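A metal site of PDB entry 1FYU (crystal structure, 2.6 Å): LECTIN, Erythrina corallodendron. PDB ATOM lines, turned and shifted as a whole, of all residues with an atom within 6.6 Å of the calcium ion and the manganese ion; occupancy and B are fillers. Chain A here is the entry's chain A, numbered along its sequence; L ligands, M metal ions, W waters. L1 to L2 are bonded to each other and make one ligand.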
ATOM      1  N   ASP A  89     -14.271   2.101   8.289  1.00  0.00           N
ATOM      2  CA  ASP A  89     -15.447   1.825   7.485  1.00  0.00           C
ATOM      3  C   ASP A  89     -15.189   0.790   6.394  1.00  0.00           C
ATOM      4  O   ASP A  89     -16.089   0.051   5.993  1.00  0.00           O
ATOM      5  CB  ASP A  89     -15.964   3.129   6.859  1.00  0.00           C
ATOM      6  CG  ASP A  89     -17.028   3.819   7.714  1.00  0.00           C
ATOM      7  OD1 ASP A  89     -16.691   4.768   8.469  1.00  0.00           O
ATOM      8  OD2 ASP A  89     -18.202   3.404   7.632  1.00  0.00           O
ATOM      9  N   TYR A 106     -16.017   8.207   5.729  1.00  0.00           N
ATOM     10  CA  TYR A 106     -16.865   7.246   6.436  1.00  0.00           C
ATOM     11  C   TYR A 106     -17.430   6.197   5.480  1.00  0.00           C
ATOM     12  O   TYR A 106     -16.704   5.675   4.634  1.00  0.00           O
ATOM     13  CB  TYR A 106     -18.004   7.964   7.171  1.00  0.00           C
ATOM     14  CG  TYR A 106     -17.539   9.165   7.959  1.00  0.00           C
ATOM     15  CD1 TYR A 106     -16.353   9.136   8.696  1.00  0.00           C
ATOM     16  CD2 TYR A 106     -18.257  10.367   7.919  1.00  0.00           C
ATOM     17  CE1 TYR A 106     -15.887  10.272   9.369  1.00  0.00           C
ATOM     18  CE2 TYR A 106     -17.802  11.511   8.587  1.00  0.00           C
ATOM     19  CZ  TYR A 106     -16.619  11.452   9.293  1.00  0.00           C
ATOM     20  OH  TYR A 106     -16.134  12.588   9.916  1.00  0.00           O
ATOM     21  N   GLY A 107     -18.715   5.892   5.624  1.00  0.00           N
ATOM     22  CA  GLY A 107     -19.355   4.893   4.792  1.00  0.00           C
ATOM     23  C   GLY A 107     -19.313   5.150   3.293  1.00  0.00           C
ATOM     24  O   GLY A 107     -19.653   4.274   2.502  1.00  0.00           O
ATOM     25  N   TYR A 108     -18.925   6.360   2.897  1.00  0.00           N
ATOM     26  CA  TYR A 108     -18.860   6.685   1.475  1.00  0.00           C
ATOM     27  C   TYR A 108     -17.489   6.298   0.922  1.00  0.00           C
ATOM     28  O   TYR A 108     -17.201   6.481  -0.264  1.00  0.00           O
ATOM     29  CB  TYR A 108     -19.152   8.174   1.273  1.00  0.00           C
ATOM     30  CG  TYR A 108     -20.527   8.536   1.787  1.00  0.00           C
ATOM     31  CD1 TYR A 108     -21.667   8.053   1.156  1.00  0.00           C
ATOM     32  CD2 TYR A 108     -20.673   9.309   2.937  1.00  0.00           C
ATOM     33  CE1 TYR A 108     -22.929   8.320   1.657  1.00  0.00           C
ATOM     34  CE2 TYR A 108     -21.941   9.581   3.454  1.00  0.00           C
ATOM     35  CZ  TYR A 108     -23.055   9.083   2.811  1.00  0.00           C
ATOM     36  OH  TYR A 108     -24.310   9.330   3.322  1.00  0.00           O
ATOM     37  N   LEU A 109     -16.657   5.752   1.809  1.00  0.00           N
ATOM     38  CA  LEU A 109     -15.319   5.269   1.472  1.00  0.00           C
ATOM     39  C   LEU A 109     -14.435   6.221   0.660  1.00  0.00           C
ATOM     40  O   LEU A 109     -13.434   5.796   0.091  1.00  0.00           O
ATOM     41  CB  LEU A 109     -15.452   3.921   0.762  1.00  0.00           C
ATOM     42  CG  LEU A 109     -16.276   2.888   1.551  1.00  0.00           C
ATOM     43  CD1 LEU A 109     -16.415   1.618   0.738  1.00  0.00           C
ATOM     44  CD2 LEU A 109     -15.620   2.585   2.887  1.00  0.00           C
ATOM     45  N   GLU A 127     -15.834  -2.979  -3.237  1.00  0.00           N
ATOM     46  CA  GLU A 127     -15.576  -2.621  -1.855  1.00  0.00           C
ATOM     47  C   GLU A 127     -15.435  -3.800  -0.888  1.00  0.00           C
ATOM     48  O   GLU A 127     -15.885  -4.926  -1.150  1.00  0.00           O
ATOM     49  CB  GLU A 127     -16.722  -1.726  -1.363  1.00  0.00           C
ATOM     50  CG  GLU A 127     -18.032  -2.487  -1.203  1.00  0.00           C
ATOM     51  CD  GLU A 127     -19.166  -1.641  -0.659  1.00  0.00           C
ATOM     52  OE1 GLU A 127     -20.057  -2.218  -0.010  1.00  0.00           O
ATOM     53  OE2 GLU A 127     -19.189  -0.413  -0.899  1.00  0.00           O
ATOM     54  N   ASP A 129     -16.349  -3.621   2.659  1.00  0.00           N
ATOM     55  CA  ASP A 129     -17.090  -2.854   3.655  1.00  0.00           C
ATOM     56  C   ASP A 129     -17.109  -3.531   5.023  1.00  0.00           C
ATOM     57  O   ASP A 129     -17.529  -4.679   5.138  1.00  0.00           O
ATOM     58  CB  ASP A 129     -18.530  -2.696   3.144  1.00  0.00           C
ATOM     59  CG  ASP A 129     -19.239  -1.539   3.768  1.00  0.00           C
ATOM     60  OD1 ASP A 129     -18.911  -1.191   4.923  1.00  0.00           O
ATOM     61  OD2 ASP A 129     -20.148  -0.979   3.125  1.00  0.00           O
ATOM     62  N   THR A 130     -16.676  -2.805   6.042  1.00  0.00           N
ATOM     63  CA  THR A 130     -16.628  -3.350   7.394  1.00  0.00           C
ATOM     64  C   THR A 130     -17.673  -2.778   8.350  1.00  0.00           C
ATOM     65  O   THR A 130     -17.750  -3.209   9.512  1.00  0.00           O
ATOM     66  CB  THR A 130     -15.241  -3.161   8.015  1.00  0.00           C
ATOM     67  OG1 THR A 130     -14.947  -1.768   8.118  1.00  0.00           O
ATOM     68  CG2 THR A 130     -14.176  -3.857   7.169  1.00  0.00           C
ATOM     69  N   PHE A 131     -18.458  -1.815   7.897  1.00  0.00           N
ATOM     70  CA  PHE A 131     -19.483  -1.216   8.737  1.00  0.00           C
ATOM     71  C   PHE A 131     -20.813  -1.165   7.992  1.00  0.00           C
ATOM     72  O   PHE A 131     -20.884  -0.750   6.844  1.00  0.00           O
ATOM     73  CB  PHE A 131     -19.075   0.183   9.180  1.00  0.00           C
ATOM     74  CG  PHE A 131     -20.068   0.847  10.095  1.00  0.00           C
ATOM     75  CD1 PHE A 131     -21.191   1.495   9.576  1.00  0.00           C
ATOM     76  CD2 PHE A 131     -19.908   0.771  11.479  1.00  0.00           C
ATOM     77  CE1 PHE A 131     -22.147   2.063  10.425  1.00  0.00           C
ATOM     78  CE2 PHE A 131     -20.860   1.341  12.341  1.00  0.00           C
ATOM     79  CZ  PHE A 131     -21.983   1.995  11.814  1.00  0.00           C
ATOM     80  N   SER A 132     -21.880  -1.572   8.671  1.00  0.00           N
ATOM     81  CA  SER A 132     -23.196  -1.594   8.057  1.00  0.00           C
ATOM     82  C   SER A 132     -23.997  -0.300   8.156  1.00  0.00           C
ATOM     83  O   SER A 132     -24.590   0.003   9.196  1.00  0.00           O
ATOM     84  CB  SER A 132     -24.015  -2.734   8.656  1.00  0.00           C
ATOM     85  OG  SER A 132     -25.235  -2.851   7.959  1.00  0.00           O
ATOM     86  N   ASN A 133     -24.021   0.459   7.061  1.00  0.00           N
ATOM     87  CA  ASN A 133     -24.761   1.707   7.018  1.00  0.00           C
ATOM     88  C   ASN A 133     -26.227   1.417   6.648  1.00  0.00           C
ATOM     89  O   ASN A 133     -26.601   0.265   6.423  1.00  0.00           O
ATOM     90  CB  ASN A 133     -24.152   2.655   5.977  1.00  0.00           C
ATOM     91  CG  ASN A 133     -22.711   2.993   6.284  1.00  0.00           C
ATOM     92  OD1 ASN A 133     -21.808   2.211   5.993  1.00  0.00           O
ATOM     93  ND2 ASN A 133     -22.480   4.156   6.876  1.00  0.00           N
ATOM     94  N   TRP A 135     -27.787   1.785   3.952  1.00  0.00           N
ATOM     95  CA  TRP A 135     -27.885   1.186   2.627  1.00  0.00           C
ATOM     96  C   TRP A 135     -27.200  -0.169   2.497  1.00  0.00           C
ATOM     97  O   TRP A 135     -27.238  -0.785   1.442  1.00  0.00           O
ATOM     98  CB  TRP A 135     -27.292   2.146   1.595  1.00  0.00           C
ATOM     99  CG  TRP A 135     -25.876   2.523   1.894  1.00  0.00           C
ATOM    100  CD1 TRP A 135     -24.757   1.774   1.641  1.00  0.00           C
ATOM    101  CD2 TRP A 135     -25.423   3.705   2.562  1.00  0.00           C
ATOM    102  NE1 TRP A 135     -23.632   2.416   2.103  1.00  0.00           N
ATOM    103  CE2 TRP A 135     -24.009   3.603   2.681  1.00  0.00           C
ATOM    104  CE3 TRP A 135     -26.056   4.838   3.080  1.00  0.00           C
ATOM    105  CZ2 TRP A 135     -23.231   4.599   3.295  1.00  0.00           C
ATOM    106  CZ3 TRP A 135     -25.279   5.835   3.695  1.00  0.00           C
ATOM    107  CH2 TRP A 135     -23.877   5.700   3.794  1.00  0.00           C
ATOM    108  N   ASP A 136     -26.577  -0.634   3.575  1.00  0.00           N
ATOM    109  CA  ASP A 136     -25.867  -1.912   3.566  1.00  0.00           C
ATOM    110  C   ASP A 136     -26.697  -3.078   4.054  1.00  0.00           C
ATOM    111  O   ASP A 136     -27.719  -2.886   4.712  1.00  0.00           O
ATOM    112  CB  ASP A 136     -24.624  -1.853   4.462  1.00  0.00           C
ATOM    113  CG  ASP A 136     -23.491  -1.079   3.848  1.00  0.00           C
ATOM    114  OD1 ASP A 136     -23.136  -1.385   2.696  1.00  0.00           O
ATOM    115  OD2 ASP A 136     -22.933  -0.186   4.523  1.00  0.00           O
ATOM    116  N   PRO A 137     -26.284  -4.300   3.712  1.00  0.00           N
ATOM    117  CA  PRO A 137     -27.016  -5.479   4.183  1.00  0.00           C
ATOM    118  C   PRO A 137     -26.596  -5.569   5.654  1.00  0.00           C
ATOM    119  O   PRO A 137     -25.693  -4.847   6.079  1.00  0.00           O
ATOM    120  CB  PRO A 137     -26.439  -6.605   3.328  1.00  0.00           C
ATOM    121  CG  PRO A 137     -25.038  -6.132   3.020  1.00  0.00           C
ATOM    122  CD  PRO A 137     -25.271  -4.681   2.705  1.00  0.00           C
ATOM    123  N   VAL A 140     -21.416  -7.824   7.925  1.00  0.00           N
ATOM    124  CA  VAL A 140     -20.143  -7.176   7.671  1.00  0.00           C
ATOM    125  C   VAL A 140     -19.048  -8.020   8.304  1.00  0.00           C
ATOM    126  O   VAL A 140     -19.265  -8.708   9.288  1.00  0.00           O
ATOM    127  CB  VAL A 140     -20.093  -5.728   8.249  1.00  0.00           C
ATOM    128  CG1 VAL A 140     -21.079  -4.841   7.502  1.00  0.00           C
ATOM    129  CG2 VAL A 140     -20.390  -5.742   9.726  1.00  0.00           C
ATOM    130  N   HIS A 142     -18.273  -7.293   4.150  1.00  0.00           N
ATOM    131  CA  HIS A 142     -18.835  -7.881   2.945  1.00  0.00           C
ATOM    132  C   HIS A 142     -18.149  -7.294   1.723  1.00  0.00           C
ATOM    133  O   HIS A 142     -17.648  -6.167   1.753  1.00  0.00           O
ATOM    134  CB  HIS A 142     -20.349  -7.651   2.859  1.00  0.00           C
ATOM    135  CG  HIS A 142     -20.761  -6.200   2.810  1.00  0.00           C
ATOM    136  ND1 HIS A 142     -21.405  -5.576   3.860  1.00  0.00           N
ATOM    137  CD2 HIS A 142     -20.632  -5.266   1.839  1.00  0.00           C
ATOM    138  CE1 HIS A 142     -21.652  -4.324   3.536  1.00  0.00           C
ATOM    139  NE2 HIS A 142     -21.197  -4.105   2.310  1.00  0.00           N
ATOM    140  N   ILE A 143     -18.103  -8.081   0.656  1.00  0.00           N
ATOM    141  CA  ILE A 143     -17.539  -7.622  -0.603  1.00  0.00           C
ATOM    142  C   ILE A 143     -18.767  -7.094  -1.322  1.00  0.00           C
ATOM    143  O   ILE A 143     -19.861  -7.656  -1.195  1.00  0.00           O
ATOM    144  CB  ILE A 143     -16.930  -8.777  -1.432  1.00  0.00           C
ATOM    145  CG1 ILE A 143     -15.916  -9.548  -0.588  1.00  0.00           C
ATOM    146  CG2 ILE A 143     -16.273  -8.225  -2.698  1.00  0.00           C
ATOM    147  CD1 ILE A 143     -15.336 -10.765  -1.299  1.00  0.00           C
ATOM    148  N   GLY A 144     -18.612  -6.005  -2.063  1.00  0.00           N
ATOM    149  CA  GLY A 144     -19.740  -5.455  -2.777  1.00  0.00           C
ATOM    150  C   GLY A 144     -19.291  -4.849  -4.086  1.00  0.00           C
ATOM    151  O   GLY A 144     -18.184  -4.306  -4.190  1.00  0.00           O
ATOM    152  N   ASP A 146     -19.908  -1.984  -6.582  1.00  0.00           N
ATOM    153  CA  ASP A 146     -20.519  -0.665  -6.638  1.00  0.00           C
ATOM    154  C   ASP A 146     -20.535  -0.037  -8.023  1.00  0.00           C
ATOM    155  O   ASP A 146     -19.478   0.253  -8.586  1.00  0.00           O
ATOM    156  CB  ASP A 146     -19.814   0.280  -5.656  1.00  0.00           C
ATOM    157  CG  ASP A 146     -19.918  -0.189  -4.217  1.00  0.00           C
ATOM    158  OD1 ASP A 146     -20.708  -1.108  -3.931  1.00  0.00           O
ATOM    159  OD2 ASP A 146     -19.212   0.383  -3.370  1.00  0.00           O
ATOM    160  N   ILE A 150     -22.943   3.789  -3.705  1.00  0.00           N
ATOM    161  CA  ILE A 150     -22.388   3.101  -2.563  1.00  0.00           C
ATOM    162  C   ILE A 150     -23.338   1.966  -2.212  1.00  0.00           C
ATOM    163  O   ILE A 150     -22.988   1.058  -1.469  1.00  0.00           O
ATOM    164  CB  ILE A 150     -22.259   4.038  -1.343  1.00  0.00           C
ATOM    165  CG1 ILE A 150     -21.387   3.389  -0.276  1.00  0.00           C
ATOM    166  CG2 ILE A 150     -23.645   4.348  -0.779  1.00  0.00           C
ATOM    167  CD1 ILE A 150     -19.951   3.136  -0.724  1.00  0.00           C
ATOM    168  N   ARG A 151     -24.555   2.021  -2.749  1.00  0.00           N
ATOM    169  CA  ARG A 151     -25.524   0.953  -2.496  1.00  0.00           C
ATOM    170  C   ARG A 151     -25.233  -0.116  -3.552  1.00  0.00           C
ATOM    171  O   ARG A 151     -25.701  -0.031  -4.687  1.00  0.00           O
ATOM    172  CB  ARG A 151     -26.961   1.477  -2.626  1.00  0.00           C
ATOM    173  CG  ARG A 151     -28.003   0.410  -2.330  1.00  0.00           C
ATOM    174  CD  ARG A 151     -29.446   0.870  -2.512  1.00  0.00           C
ATOM    175  NE  ARG A 151     -30.054   1.390  -1.295  1.00  0.00           N
ATOM    176  CZ  ARG A 151     -30.001   2.666  -0.900  1.00  0.00           C
ATOM    177  NH1 ARG A 151     -29.363   3.566  -1.640  1.00  0.00           N
ATOM    178  NH2 ARG A 151     -30.588   3.030   0.238  1.00  0.00           N
ATOM    179  N   SER A 152     -24.429  -1.106  -3.168  1.00  0.00           N
ATOM    180  CA  SER A 152     -24.006  -2.203  -4.038  1.00  0.00           C
ATOM    181  C   SER A 152     -25.127  -2.908  -4.780  1.00  0.00           C
ATOM    182  O   SER A 152     -26.223  -3.052  -4.250  1.00  0.00           O
ATOM    183  CB  SER A 152     -23.249  -3.247  -3.218  1.00  0.00           C
ATOM    184  OG  SER A 152     -22.158  -2.680  -2.515  1.00  0.00           O
ATOM    185  N   THR A 155     -23.818  -8.208  -3.283  1.00  0.00           N
ATOM    186  CA  THR A 155     -23.091  -8.286  -2.035  1.00  0.00           C
ATOM    187  C   THR A 155     -22.724  -9.713  -1.620  1.00  0.00           C
ATOM    188  O   THR A 155     -23.495 -10.647  -1.860  1.00  0.00           O
ATOM    189  CB  THR A 155     -23.942  -7.601  -0.940  1.00  0.00           C
ATOM    190  OG1 THR A 155     -23.378  -6.325  -0.651  1.00  0.00           O
ATOM    191  CG2 THR A 155     -24.051  -8.450   0.300  1.00  0.00           C
HETATM  192  C1  LIG L   1     -23.693  10.027  14.869  1.00  0.00           C
HETATM  193  C2  LIG L   1     -22.530   9.115  15.273  1.00  0.00           C
HETATM  194  C3  LIG L   1     -21.686   8.774  14.043  1.00  0.00           C
HETATM  195  C4  LIG L   1     -22.563   8.181  12.934  1.00  0.00           C
HETATM  196  C5  LIG L   1     -23.784   9.075  12.656  1.00  0.00           C
HETATM  197  C6  LIG L   1     -24.776   8.385  11.733  1.00  0.00           C
HETATM  198  O1  LIG L   1     -23.191  11.187  14.287  1.00  0.00           O
HETATM  199  O2  LIG L   1     -21.725   9.773  16.240  1.00  0.00           O
HETATM  200  O3  LIG L   1     -20.686   7.835  14.408  1.00  0.00           O
HETATM  201  O4  LIG L   1     -21.788   8.027  11.724  1.00  0.00           O
HETATM  202  O5  LIG L   1     -24.505   9.358  13.885  1.00  0.00           O
HETATM  203  O6  LIG L   1     -25.264   9.289  10.761  1.00  0.00           O
HETATM  204  C1  LG2 L   2     -21.460   6.719  11.371  1.00  0.00           C
HETATM  205  C2  LG2 L   2     -21.003   6.680   9.905  1.00  0.00           C
HETATM  206  C3  LG2 L   2     -20.501   5.262   9.548  1.00  0.00           C
HETATM  207  C4  LG2 L   2     -19.445   4.795  10.550  1.00  0.00           C
HETATM  208  C5  LG2 L   2     -20.000   4.913  11.968  1.00  0.00           C
HETATM  209  C6  LG2 L   2     -18.993   4.536  13.033  1.00  0.00           C
HETATM  210  O1  LG2 L   2     -22.089   7.036   9.061  1.00  0.00           O
HETATM  211  O2  LG2 L   2     -19.943   5.268   8.246  1.00  0.00           O
HETATM  212  O3  LG2 L   2     -18.284   5.604  10.422  1.00  0.00           O
HETATM  213  O4  LG2 L   2     -20.398   6.290  12.229  1.00  0.00           O
HETATM  214  O5  LG2 L   2     -19.516   4.743  14.327  1.00  0.00           O
HETATM  215 CA    CA M   1     -20.745   0.517   4.929  1.00  0.00          CA
HETATM  216 MN    MN M   2     -21.487  -1.931   1.597  1.00  0.00          MN
HETATM  217  O   HOH W   1     -20.541   1.849   2.870  1.00  0.00           O
HETATM  218  O   HOH W   2     -18.787   1.629   5.669  1.00  0.00           O
HETATM  219  O   HOH W   3     -21.284   0.164   0.776  1.00  0.00           O
HETATM  220  O   HOH W   4     -22.892  -2.514   0.110  1.00  0.00           O
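The calcium ion is bound by OD1 of Asn 133 (2.3 Å), O of Phe 131 (2.3 Å), OD2 of Asp 136 (2.3 Å), water W2 (2.4 Å), OD2 of Asp 129 (2.4 Å), water W1 (2.5 Å) and OD1 of Asp 129 (2.5 Å).
The calcium ion has seven donor atoms within binding distance.
The manganese ion is bound by OD1 of Asp 136 (2.1 Å), water W4 (2.1 Å), OE1 of Glu 127 (2.2 Å), OD2 of Asp 129 (2.2 Å), water W3 (2.3 Å) and NE2 of His 142 (2.3 Å).
The side-chain carboxylate of Asp 89 sits at hydrogen-bond distance from an oxygen (O2) of LG2 L2 (2.6 Å).
An oxygen (O2) of LG2 L2 lies within hydrogen-bond range of the side-chain amide nitrogen (ND2) of Asn 133, at 3.1 Å.
N of Gly 107 lies within hydrogen-bond range of O2 of LG2 L2 (3.0 Å).
The nearest printed residue that does not touch the manganese ion is Ser 152 (4.2 Å).
Water W1 bridges the backbone carbonyl oxygen of Gly 107 and the indole nitrogen of Trp 135.
Water W3 bridges the side-chain carboxylate (OE2) of Glu 127 and the backbone carbonyl oxygen (O) of Ile 150.
Four residues have an atom within 4 Å of the calcium ion: Asp 129, Phe 131, Asn 133 and Asp 136.
The nearest printed residue that does not touch the calcium ion is Ser 132 (4.4 Å).
O of Gly 144 is in hydrogen-bond range of N of Glu 127 (2.9 Å).
The side-chain carboxylate (OE2) of Glu 127 sits close to the side-chain carboxylate (OD2) of Asp 146 (2.6 Å).
The side-chain hydroxyl of Ser 152 lies close to the side-chain carboxylate of Glu 127 (3.3 Å).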
